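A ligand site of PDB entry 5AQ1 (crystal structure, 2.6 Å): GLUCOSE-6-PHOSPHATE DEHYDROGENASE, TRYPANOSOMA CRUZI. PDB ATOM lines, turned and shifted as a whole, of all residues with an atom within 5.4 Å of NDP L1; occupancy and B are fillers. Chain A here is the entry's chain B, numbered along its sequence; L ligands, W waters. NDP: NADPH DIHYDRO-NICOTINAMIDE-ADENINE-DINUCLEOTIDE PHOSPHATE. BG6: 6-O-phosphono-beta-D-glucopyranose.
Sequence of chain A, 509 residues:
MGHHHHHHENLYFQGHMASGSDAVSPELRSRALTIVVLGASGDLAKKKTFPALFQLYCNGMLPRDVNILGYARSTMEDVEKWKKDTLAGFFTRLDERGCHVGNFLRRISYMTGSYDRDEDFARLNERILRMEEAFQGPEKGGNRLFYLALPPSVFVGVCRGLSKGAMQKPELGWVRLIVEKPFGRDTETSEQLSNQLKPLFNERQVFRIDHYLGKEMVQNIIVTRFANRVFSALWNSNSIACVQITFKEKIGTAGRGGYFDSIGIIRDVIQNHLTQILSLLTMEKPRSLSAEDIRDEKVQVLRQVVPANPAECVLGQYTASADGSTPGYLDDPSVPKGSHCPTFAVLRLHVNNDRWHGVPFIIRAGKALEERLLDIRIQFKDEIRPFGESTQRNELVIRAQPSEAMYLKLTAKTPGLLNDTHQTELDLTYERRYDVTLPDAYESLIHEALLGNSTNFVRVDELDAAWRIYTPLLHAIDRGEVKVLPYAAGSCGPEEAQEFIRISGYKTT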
ATOM      1  N   GLY A  39       2.787   1.436 -13.982  1.00  0.00           N
ATOM      2  CA  GLY A  39       1.671   0.602 -13.557  1.00  0.00           C
ATOM      3  C   GLY A  39       1.991  -0.084 -12.233  1.00  0.00           C
ATOM      4  O   GLY A  39       1.592  -1.221 -12.010  1.00  0.00           O
ATOM      5  N   SER A  41       0.888   0.331  -9.331  1.00  0.00           N
ATOM      6  CA  SER A  41      -0.302   0.035  -8.541  1.00  0.00           C
ATOM      7  C   SER A  41      -1.021  -1.256  -8.979  1.00  0.00           C
ATOM      8  O   SER A  41      -2.058  -1.601  -8.429  1.00  0.00           O
ATOM      9  CB  SER A  41      -1.285   1.199  -8.646  1.00  0.00           C
ATOM     10  OG  SER A  41      -1.633   1.435  -9.999  1.00  0.00           O
ATOM     11  N   GLY A  42      -0.450  -1.983  -9.948  1.00  0.00           N
ATOM     12  CA  GLY A  42      -1.134  -3.095 -10.597  1.00  0.00           C
ATOM     13  C   GLY A  42      -0.872  -4.469 -10.014  1.00  0.00           C
ATOM     14  O   GLY A  42      -0.107  -4.636  -9.073  1.00  0.00           O
ATOM     15  N   ASP A  43      -1.539  -5.456 -10.620  1.00  0.00           N
ATOM     16  CA  ASP A  43      -1.479  -6.831 -10.151  1.00  0.00           C
ATOM     17  C   ASP A  43      -0.099  -7.448 -10.347  1.00  0.00           C
ATOM     18  O   ASP A  43       0.472  -8.032  -9.424  1.00  0.00           O
ATOM     19  CB  ASP A  43      -2.525  -7.680 -10.876  1.00  0.00           C
ATOM     20  CG  ASP A  43      -2.772  -9.014 -10.212  1.00  0.00           C
ATOM     21  OD1 ASP A  43      -3.315  -9.019  -9.092  1.00  0.00           O
ATOM     22  OD2 ASP A  43      -2.406 -10.058 -10.811  1.00  0.00           O
ATOM     23  N   LEU A  44       0.447  -7.303 -11.560  1.00  0.00           N
ATOM     24  CA  LEU A  44       1.768  -7.847 -11.877  1.00  0.00           C
ATOM     25  C   LEU A  44       2.858  -7.193 -11.030  1.00  0.00           C
ATOM     26  O   LEU A  44       3.768  -7.876 -10.557  1.00  0.00           O
ATOM     27  CB  LEU A  44       2.080  -7.647 -13.360  1.00  0.00           C
ATOM     28  CG  LEU A  44       3.427  -8.194 -13.860  1.00  0.00           C
ATOM     29  CD1 LEU A  44       3.443  -9.715 -13.799  1.00  0.00           C
ATOM     30  CD2 LEU A  44       3.715  -7.717 -15.271  1.00  0.00           C
ATOM     31  N   ALA A  45       2.762  -5.878 -10.857  1.00  0.00           N
ATOM     32  CA  ALA A  45       3.756  -5.121 -10.112  1.00  0.00           C
ATOM     33  C   ALA A  45       3.983  -5.687  -8.702  1.00  0.00           C
ATOM     34  O   ALA A  45       5.115  -6.007  -8.332  1.00  0.00           O
ATOM     35  CB  ALA A  45       3.371  -3.659 -10.047  1.00  0.00           C
ATOM     36  N   LYS A  48       4.702  -9.915  -8.782  1.00  0.00           N
ATOM     37  CA  LYS A  48       5.884 -10.426  -9.479  1.00  0.00           C
ATOM     38  C   LYS A  48       7.052  -9.436  -9.538  1.00  0.00           C
ATOM     39  O   LYS A  48       8.171  -9.776  -9.147  1.00  0.00           O
ATOM     40  CB  LYS A  48       5.503 -10.865 -10.894  1.00  0.00           C
ATOM     41  CG  LYS A  48       4.557 -12.053 -10.939  1.00  0.00           C
ATOM     42  CD  LYS A  48       5.174 -13.278 -10.274  1.00  0.00           C
ATOM     43  CE  LYS A  48       4.327 -14.525 -10.444  1.00  0.00           C
ATOM     44  NZ  LYS A  48       4.836 -15.627  -9.573  1.00  0.00           N
ATOM     45  N   ALA A  72       2.209   5.577 -11.757  1.00  0.00           N
ATOM     46  CA  ALA A  72       0.841   5.237 -12.145  1.00  0.00           C
ATOM     47  C   ALA A  72      -0.114   6.415 -11.890  1.00  0.00           C
ATOM     48  O   ALA A  72       0.275   7.404 -11.275  1.00  0.00           O
ATOM     49  CB  ALA A  72       0.370   3.998 -11.398  1.00  0.00           C
ATOM     50  N   ARG A  73      -1.352   6.283 -12.357  1.00  0.00           N
ATOM     51  CA  ARG A  73      -2.348   7.342 -12.223  1.00  0.00           C
ATOM     52  C   ARG A  73      -2.904   7.464 -10.812  1.00  0.00           C
ATOM     53  O   ARG A  73      -3.344   8.545 -10.405  1.00  0.00           O
ATOM     54  CB  ARG A  73      -3.513   7.122 -13.189  1.00  0.00           C
ATOM     55  CG  ARG A  73      -3.110   7.062 -14.666  1.00  0.00           C
ATOM     56  CD  ARG A  73      -4.286   6.659 -15.538  1.00  0.00           C
ATOM     57  NE  ARG A  73      -4.881   5.411 -15.084  1.00  0.00           N
ATOM     58  CZ  ARG A  73      -6.089   4.971 -15.438  1.00  0.00           C
ATOM     59  NH1 ARG A  73      -6.857   5.674 -16.268  1.00  0.00           N
ATOM     60  NH2 ARG A  73      -6.539   3.814 -14.963  1.00  0.00           N
ATOM     61  N   SER A  74      -2.911   6.355 -10.061  1.00  0.00           N
ATOM     62  CA  SER A  74      -3.422   6.339  -8.693  1.00  0.00           C
ATOM     63  C   SER A  74      -2.640   7.291  -7.792  1.00  0.00           C
ATOM     64  O   SER A  74      -1.418   7.390  -7.897  1.00  0.00           O
ATOM     65  CB  SER A  74      -3.366   4.926  -8.098  1.00  0.00           C
ATOM     66  OG  SER A  74      -4.336   4.077  -8.692  1.00  0.00           O
ATOM     67  N   TYR A 110       7.430   6.464  -5.131  1.00  0.00           N
ATOM     68  CA  TYR A 110       6.217   6.450  -5.945  1.00  0.00           C
ATOM     69  C   TYR A 110       5.936   7.850  -6.484  1.00  0.00           C
ATOM     70  O   TYR A 110       6.340   8.851  -5.897  1.00  0.00           O
ATOM     71  CB  TYR A 110       5.010   5.916  -5.174  1.00  0.00           C
ATOM     72  CG  TYR A 110       3.768   5.798  -6.028  1.00  0.00           C
ATOM     73  CD1 TYR A 110       3.569   4.694  -6.853  1.00  0.00           C
ATOM     74  CD2 TYR A 110       2.803   6.801  -6.041  1.00  0.00           C
ATOM     75  CE1 TYR A 110       2.447   4.590  -7.647  1.00  0.00           C
ATOM     76  CE2 TYR A 110       1.682   6.704  -6.843  1.00  0.00           C
ATOM     77  CZ  TYR A 110       1.499   5.595  -7.643  1.00  0.00           C
ATOM     78  OH  TYR A 110       0.377   5.506  -8.438  1.00  0.00           O
ATOM     79  N   TYR A 115      -0.640   8.339 -18.585  1.00  0.00           N
ATOM     80  CA  TYR A 115       0.095   7.517 -19.541  1.00  0.00           C
ATOM     81  C   TYR A 115       0.104   8.116 -20.963  1.00  0.00           C
ATOM     82  O   TYR A 115       0.604   7.476 -21.897  1.00  0.00           O
ATOM     83  CB  TYR A 115      -0.516   6.109 -19.583  1.00  0.00           C
ATOM     84  CG  TYR A 115      -0.514   5.390 -18.250  1.00  0.00           C
ATOM     85  CD1 TYR A 115       0.667   5.209 -17.541  1.00  0.00           C
ATOM     86  CD2 TYR A 115      -1.696   4.878 -17.708  1.00  0.00           C
ATOM     87  CE1 TYR A 115       0.680   4.543 -16.319  1.00  0.00           C
ATOM     88  CE2 TYR A 115      -1.691   4.218 -16.495  1.00  0.00           C
ATOM     89  CZ  TYR A 115      -0.507   4.057 -15.809  1.00  0.00           C
ATOM     90  OH  TYR A 115      -0.512   3.396 -14.598  1.00  0.00           O
ATOM     91  N   LEU A 148       7.198  -1.822 -18.260  1.00  0.00           N
ATOM     92  CA  LEU A 148       5.826  -1.476 -18.610  1.00  0.00           C
ATOM     93  C   LEU A 148       4.863  -2.552 -18.138  1.00  0.00           C
ATOM     94  O   LEU A 148       4.501  -3.448 -18.907  1.00  0.00           O
ATOM     95  CB  LEU A 148       5.683  -1.245 -20.117  1.00  0.00           C
ATOM     96  CG  LEU A 148       6.073   0.167 -20.598  1.00  0.00           C
ATOM     97  CD1 LEU A 148       7.514   0.503 -20.267  1.00  0.00           C
ATOM     98  CD2 LEU A 148       5.830   0.291 -22.095  1.00  0.00           C
ATOM     99  N   ALA A 149       4.451  -2.462 -16.876  1.00  0.00           N
ATOM    100  CA  ALA A 149       3.460  -3.371 -16.295  1.00  0.00           C
ATOM    101  C   ALA A 149       2.061  -2.795 -16.453  1.00  0.00           C
ATOM    102  O   ALA A 149       1.361  -2.539 -15.468  1.00  0.00           O
ATOM    103  CB  ALA A 149       3.772  -3.610 -14.818  1.00  0.00           C
ATOM    104  N   LEU A 150       1.644  -2.616 -17.708  1.00  0.00           N
ATOM    105  CA  LEU A 150       0.433  -1.892 -18.066  1.00  0.00           C
ATOM    106  C   LEU A 150      -0.434  -2.709 -19.025  1.00  0.00           C
ATOM    107  O   LEU A 150       0.056  -3.633 -19.660  1.00  0.00           O
ATOM    108  CB  LEU A 150       0.820  -0.579 -18.764  1.00  0.00           C
ATOM    109  CG  LEU A 150       1.681   0.402 -17.958  1.00  0.00           C
ATOM    110  CD1 LEU A 150       2.330   1.421 -18.887  1.00  0.00           C
ATOM    111  CD2 LEU A 150       0.847   1.103 -16.895  1.00  0.00           C
ATOM    112  N   PRO A 151      -1.729  -2.362 -19.149  1.00  0.00           N
ATOM    113  CA  PRO A 151      -2.583  -3.020 -20.157  1.00  0.00           C
ATOM    114  C   PRO A 151      -2.183  -2.658 -21.593  1.00  0.00           C
ATOM    115  O   PRO A 151      -1.587  -1.601 -21.812  1.00  0.00           O
ATOM    116  CB  PRO A 151      -3.992  -2.486 -19.850  1.00  0.00           C
ATOM    117  CG  PRO A 151      -3.905  -1.765 -18.549  1.00  0.00           C
ATOM    118  CD  PRO A 151      -2.479  -1.357 -18.358  1.00  0.00           C
ATOM    119  N   PRO A 152      -2.524  -3.523 -22.571  1.00  0.00           N
ATOM    120  CA  PRO A 152      -2.199  -3.252 -23.978  1.00  0.00           C
ATOM    121  C   PRO A 152      -2.835  -1.983 -24.556  1.00  0.00           C
ATOM    122  O   PRO A 152      -2.291  -1.399 -25.490  1.00  0.00           O
ATOM    123  CB  PRO A 152      -2.727  -4.496 -24.714  1.00  0.00           C
ATOM    124  CG  PRO A 152      -3.609  -5.211 -23.751  1.00  0.00           C
ATOM    125  CD  PRO A 152      -3.125  -4.859 -22.378  1.00  0.00           C
ATOM    126  N   SER A 153      -3.981  -1.557 -24.019  1.00  0.00           N
ATOM    127  CA  SER A 153      -4.665  -0.351 -24.500  1.00  0.00           C
ATOM    128  C   SER A 153      -3.807   0.922 -24.438  1.00  0.00           C
ATOM    129  O   SER A 153      -3.894   1.760 -25.329  1.00  0.00           O
ATOM    130  CB  SER A 153      -5.973  -0.133 -23.731  1.00  0.00           C
ATOM    131  OG  SER A 153      -5.737  -0.047 -22.335  1.00  0.00           O
ATOM    132  N   VAL A 154      -2.981   1.057 -23.404  1.00  0.00           N
ATOM    133  CA  VAL A 154      -2.154   2.254 -23.225  1.00  0.00           C
ATOM    134  C   VAL A 154      -0.709   2.107 -23.727  1.00  0.00           C
ATOM    135  O   VAL A 154       0.051   3.071 -23.679  1.00  0.00           O
ATOM    136  CB  VAL A 154      -2.114   2.714 -21.744  1.00  0.00           C
ATOM    137  CG1 VAL A 154      -3.521   2.805 -21.165  1.00  0.00           C
ATOM    138  CG2 VAL A 154      -1.238   1.787 -20.901  1.00  0.00           C
ATOM    139  N   GLU A 180       5.306  -6.429 -21.764  1.00  0.00           N
ATOM    140  CA  GLU A 180       4.566  -7.651 -21.458  1.00  0.00           C
ATOM    141  C   GLU A 180       3.542  -7.979 -22.545  1.00  0.00           C
ATOM    142  O   GLU A 180       3.096  -7.104 -23.281  1.00  0.00           O
ATOM    143  CB  GLU A 180       3.850  -7.517 -20.117  1.00  0.00           C
ATOM    144  CG  GLU A 180       4.768  -7.527 -18.898  1.00  0.00           C
ATOM    145  CD  GLU A 180       5.157  -8.918 -18.439  1.00  0.00           C
ATOM    146  OE1 GLU A 180       4.457  -9.908 -18.776  1.00  0.00           O
ATOM    147  OE2 GLU A 180       6.166  -9.028 -17.700  1.00  0.00           O
ATOM    148  N   LYS A 181       3.155  -9.257 -22.611  1.00  0.00           N
ATOM    149  CA  LYS A 181       2.125  -9.719 -23.535  1.00  0.00           C
ATOM    150  C   LYS A 181       0.755  -9.262 -23.010  1.00  0.00           C
ATOM    151  O   LYS A 181       0.658  -8.905 -21.837  1.00  0.00           O
ATOM    152  CB  LYS A 181       2.195 -11.245 -23.694  1.00  0.00           C
ATOM    153  CG  LYS A 181       1.636 -12.064 -22.540  1.00  0.00           C
ATOM    154  CD  LYS A 181       1.872 -13.551 -22.770  1.00  0.00           C
ATOM    155  CE  LYS A 181       1.348 -14.414 -21.633  1.00  0.00           C
ATOM    156  NZ  LYS A 181      -0.118 -14.648 -21.711  1.00  0.00           N
ATOM    157  N   PRO A 182      -0.294  -9.253 -23.828  1.00  0.00           N
ATOM    158  CA  PRO A 182      -0.301  -9.725 -25.222  1.00  0.00           C
ATOM    159  C   PRO A 182       0.402  -8.802 -26.197  1.00  0.00           C
ATOM    160  O   PRO A 182       0.389  -7.570 -26.013  1.00  0.00           O
ATOM    161  CB  PRO A 182      -1.794  -9.771 -25.554  1.00  0.00           C
ATOM    162  CG  PRO A 182      -2.393  -8.695 -24.716  1.00  0.00           C
ATOM    163  CD  PRO A 182      -1.601  -8.694 -23.430  1.00  0.00           C
ATOM    164  N   TYR A 259     -11.803 -11.146 -19.321  1.00  0.00           N
ATOM    165  CA  TYR A 259     -10.612 -10.769 -20.081  1.00  0.00           C
ATOM    166  C   TYR A 259     -10.115 -11.914 -20.956  1.00  0.00           C
ATOM    167  O   TYR A 259      -9.576 -11.701 -22.045  1.00  0.00           O
ATOM    168  CB  TYR A 259      -9.506 -10.323 -19.119  1.00  0.00           C
ATOM    169  CG  TYR A 259      -8.211  -9.928 -19.793  1.00  0.00           C
ATOM    170  CD1 TYR A 259      -8.170  -8.869 -20.700  1.00  0.00           C
ATOM    171  CD2 TYR A 259      -7.027 -10.610 -19.510  1.00  0.00           C
ATOM    172  CE1 TYR A 259      -6.978  -8.506 -21.313  1.00  0.00           C
ATOM    173  CE2 TYR A 259      -5.835 -10.247 -20.124  1.00  0.00           C
ATOM    174  CZ  TYR A 259      -5.815  -9.195 -21.026  1.00  0.00           C
ATOM    175  OH  TYR A 259      -4.625  -8.831 -21.626  1.00  0.00           O
ATOM    176  N   TYR A 442      10.851 -14.114 -12.995  1.00  0.00           N
ATOM    177  CA  TYR A 442      11.119 -12.698 -13.176  1.00  0.00           C
ATOM    178  C   TYR A 442      12.429 -12.200 -12.531  1.00  0.00           C
ATOM    179  O   TYR A 442      12.905 -11.114 -12.864  1.00  0.00           O
ATOM    180  CB  TYR A 442       9.929 -11.866 -12.698  1.00  0.00           C
ATOM    181  CG  TYR A 442       8.767 -11.873 -13.669  1.00  0.00           C
ATOM    182  CD1 TYR A 442       8.787 -11.086 -14.823  1.00  0.00           C
ATOM    183  CD2 TYR A 442       7.638 -12.655 -13.439  1.00  0.00           C
ATOM    184  CE1 TYR A 442       7.730 -11.076 -15.708  1.00  0.00           C
ATOM    185  CE2 TYR A 442       6.562 -12.660 -14.327  1.00  0.00           C
ATOM    186  CZ  TYR A 442       6.618 -11.870 -15.459  1.00  0.00           C
ATOM    187  OH  TYR A 442       5.562 -11.853 -16.352  1.00  0.00           O
HETATM  188  PA  NDP L   1      -3.788  -4.505 -14.321  1.00  0.00           P
HETATM  189  O1A NDP L   1      -5.178  -4.698 -14.880  1.00  0.00           O
HETATM  190  O2A NDP L   1      -3.508  -4.824 -12.865  1.00  0.00           O
HETATM  191  O5B NDP L   1      -3.359  -2.994 -14.659  1.00  0.00           O
HETATM  192  C5B NDP L   1      -2.069  -2.520 -14.262  1.00  0.00           C
HETATM  193  C4B NDP L   1      -2.148  -1.061 -13.845  1.00  0.00           C
HETATM  194  O4B NDP L   1      -2.379  -0.267 -15.022  1.00  0.00           O
HETATM  195  C3B NDP L   1      -3.277  -0.728 -12.868  1.00  0.00           C
HETATM  196  O3B NDP L   1      -2.859  -0.726 -11.499  1.00  0.00           O
HETATM  197  C2B NDP L   1      -3.722   0.643 -13.300  1.00  0.00           C
HETATM  198  O2B NDP L   1      -2.997   1.641 -12.581  1.00  0.00           O
HETATM  199  C1B NDP L   1      -3.376   0.724 -14.773  1.00  0.00           C
HETATM  200  N9A NDP L   1      -4.590   0.524 -15.599  1.00  0.00           N
HETATM  201  C8A NDP L   1      -5.478  -0.500 -15.508  1.00  0.00           C
HETATM  202  N7A NDP L   1      -6.473  -0.350 -16.422  1.00  0.00           N
HETATM  203  C5A NDP L   1      -6.222   0.776 -17.117  1.00  0.00           C
HETATM  204  C6A NDP L   1      -6.853   1.512 -18.226  1.00  0.00           C
HETATM  205  N6A NDP L   1      -7.999   1.054 -18.783  1.00  0.00           N
HETATM  206  N1A NDP L   1      -6.260   2.655 -18.649  1.00  0.00           N
HETATM  207  C2A NDP L   1      -5.121   3.126 -18.109  1.00  0.00           C
HETATM  208  N3A NDP L   1      -4.495   2.494 -17.097  1.00  0.00           N
HETATM  209  C4A NDP L   1      -4.976   1.341 -16.571  1.00  0.00           C
HETATM  210  O3  NDP L   1      -2.721  -5.275 -15.257  1.00  0.00           O
HETATM  211  PN  NDP L   1      -1.764  -6.457 -14.722  1.00  0.00           P
HETATM  212  O1N NDP L   1      -0.825  -5.934 -13.655  1.00  0.00           O
HETATM  213  O2N NDP L   1      -2.623  -7.661 -14.435  1.00  0.00           O
HETATM  214  O5D NDP L   1      -0.884  -6.762 -16.035  1.00  0.00           O
HETATM  215  C5D NDP L   1       0.035  -5.801 -16.570  1.00  0.00           C
HETATM  216  C4D NDP L   1       0.550  -6.300 -17.912  1.00  0.00           C
HETATM  217  O4D NDP L   1       1.227  -7.557 -17.740  1.00  0.00           O
HETATM  218  C3D NDP L   1      -0.580  -6.542 -18.891  1.00  0.00           C
HETATM  219  O3D NDP L   1      -0.209  -6.118 -20.201  1.00  0.00           O
HETATM  220  C2D NDP L   1      -0.793  -8.043 -18.865  1.00  0.00           C
HETATM  221  O2D NDP L   1      -1.330  -8.539 -20.105  1.00  0.00           O
HETATM  222  C1D NDP L   1       0.600  -8.575 -18.538  1.00  0.00           C
HETATM  223  N1N NDP L   1       0.542  -9.875 -17.853  1.00  0.00           N
HETATM  224  C2N NDP L   1       0.270  -9.956 -16.539  1.00  0.00           C
HETATM  225  C3N NDP L   1       0.203 -11.173 -15.878  1.00  0.00           C
HETATM  226  C7N NDP L   1      -0.093 -11.232 -14.404  1.00  0.00           C
HETATM  227  O7N NDP L   1       0.437 -12.104 -13.731  1.00  0.00           O
HETATM  228  N7N NDP L   1      -0.933 -10.351 -13.852  1.00  0.00           N
HETATM  229  C4N NDP L   1       0.443 -12.467 -16.618  1.00  0.00           C
HETATM  230  C5N NDP L   1       0.731 -12.247 -18.035  1.00  0.00           C
HETATM  231  C6N NDP L   1       0.775 -10.977 -18.590  1.00  0.00           C
HETATM  232  P2B NDP L   1      -3.515   3.142 -12.374  1.00  0.00           P
HETATM  233  O1X NDP L   1      -5.019   3.097 -12.549  1.00  0.00           O
HETATM  234  O2X NDP L   1      -3.076   3.426 -10.961  1.00  0.00           O
HETATM  235  O3X NDP L   1      -2.808   3.950 -13.447  1.00  0.00           O
HETATM  236  C1  BG6 L   2       0.363 -16.169 -17.895  1.00  0.00           C
HETATM  237  C2  BG6 L   2      -0.987 -16.475 -18.529  1.00  0.00           C
HETATM  238  O1  BG6 L   2       1.277 -15.669 -18.875  1.00  0.00           O
HETATM  239  O5  BG6 L   2       0.905 -17.362 -17.321  1.00  0.00           O
HETATM  240  C3  BG6 L   2      -1.921 -17.070 -17.486  1.00  0.00           C
HETATM  241  O2  BG6 L   2      -1.565 -15.281 -19.082  1.00  0.00           O
HETATM  242  C4  BG6 L   2      -1.259 -18.308 -16.891  1.00  0.00           C
HETATM  243  O3  BG6 L   2      -3.192 -17.417 -18.050  1.00  0.00           O
HETATM  244  C5  BG6 L   2       0.085 -17.927 -16.286  1.00  0.00           C
HETATM  245  O4  BG6 L   2      -2.120 -18.879 -15.908  1.00  0.00           O
HETATM  246  C6  BG6 L   2       0.770 -19.134 -15.660  1.00  0.00           C
HETATM  247  O6  BG6 L   2       2.108 -18.801 -15.270  1.00  0.00           O
HETATM  248  P   BG6 L   2       2.914 -19.772 -14.277  1.00  0.00           P
HETATM  249  O1P BG6 L   2       2.877 -21.128 -14.945  1.00  0.00           O
HETATM  250  O2P BG6 L   2       4.301 -19.193 -14.225  1.00  0.00           O
HETATM  251  O3P BG6 L   2       2.149 -19.686 -12.985  1.00  0.00           O
HETATM  252  O   HOH W   1       1.131  -4.099 -12.824  1.00  0.00           O
HETATM  253  O   HOH W   2       3.297 -13.754 -17.966  1.00  0.00           O
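Merely in contact with NDP L1: Pro 182 (3.3 Å), Val 154 (3.5 Å), Pro 151 (3.5 Å), Ala 72 (3.5 Å), Glu 180 (3.5 Å), Ala 149 (3.6 Å), Tyr 259 (3.6 Å) and Pro 152 (3.9 Å).
Hydrophobic or aromatic side chains within 4 Å of NDP L1: Leu 44, Ala 72, Tyr 115, Leu 150, Pro 151, Pro 152, Val 154 and Pro 182.
Of the 24 residues printed, 17 come within 4 Å of NDP L1.
The nearest printed residue that does not touch NDP L1 is Gly 39 (4.2 Å).
O of Leu 150 is in hydrogen-bond range of O3D of NDP L1 (2.6 Å).
The side-chain hydroxyl of Ser 74 lies within hydrogen-bond range of an oxygen (O2X) of NDP L1.
The backbone NH (N) of Gly 42 lies close to an oxygen (O3B) of NDP L1 (3.1 Å).
O2 of BG6 L2 sits at hydrogen-bond distance from NZ of Lys 181, at 3.1 Å.
O of Ser 41 lies close to O3B of NDP L1 (3.3 Å).
The side-chain carboxylate (OD2) of Asp 43 is in hydrogen-bond range of a nitrogen (N7N) of NDP L1.
N of Ser 74 sits at hydrogen-bond distance from O2X of NDP L1 (3.1 Å).
The side-chain hydroxyl of Ser 41 lies within hydrogen-bond range of an oxygen (O2X) of NDP L1.
O2A of NDP L1 is in hydrogen-bond range of N of Asp 43 (3.1 Å).
The guanidinium group of Arg 73 is in salt-bridge range of an oxygen (O1X) of NDP L1, 2.9 Å away.
The backbone NH (N) of Leu 44 is in hydrogen-bond range of an oxygen (O1N) of NDP L1 (2.8 Å).
N of Arg 73 sits at hydrogen-bond distance from O3X of NDP L1, at 3.0 Å.
OH of Tyr 115 is in hydrogen-bond range of O3X of NDP L1 (2.6 Å).
The backbone carbonyl oxygen of Lys 181 is in hydrogen-bond range of an oxygen (O2D) of NDP L1 (2.7 Å).
Water W1 lies within hydrogen-bond range of O1N of NDP L1 (2.8 Å), O of Gly 39 (3.0 Å), O of Ala 149 (3.1 Å) and N of Ala 45 (3.1 Å).
Water W2 lies within hydrogen-bond range of an oxygen (O1) of BG6 L2 (2.9 Å) and the side-chain hydroxyl (OH) of Tyr 442 (3.4 Å).
OH of Tyr 110 is in hydrogen-bond range of O of Ser 74 (2.7 Å).
The side-chain carboxylate (OE2) of Glu 180 sits at hydrogen-bond distance from the side-chain hydroxyl (OH) of Tyr 442 (3.2 Å).
O of Ala 72 lies close to OH of Tyr 110 (3.4 Å).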
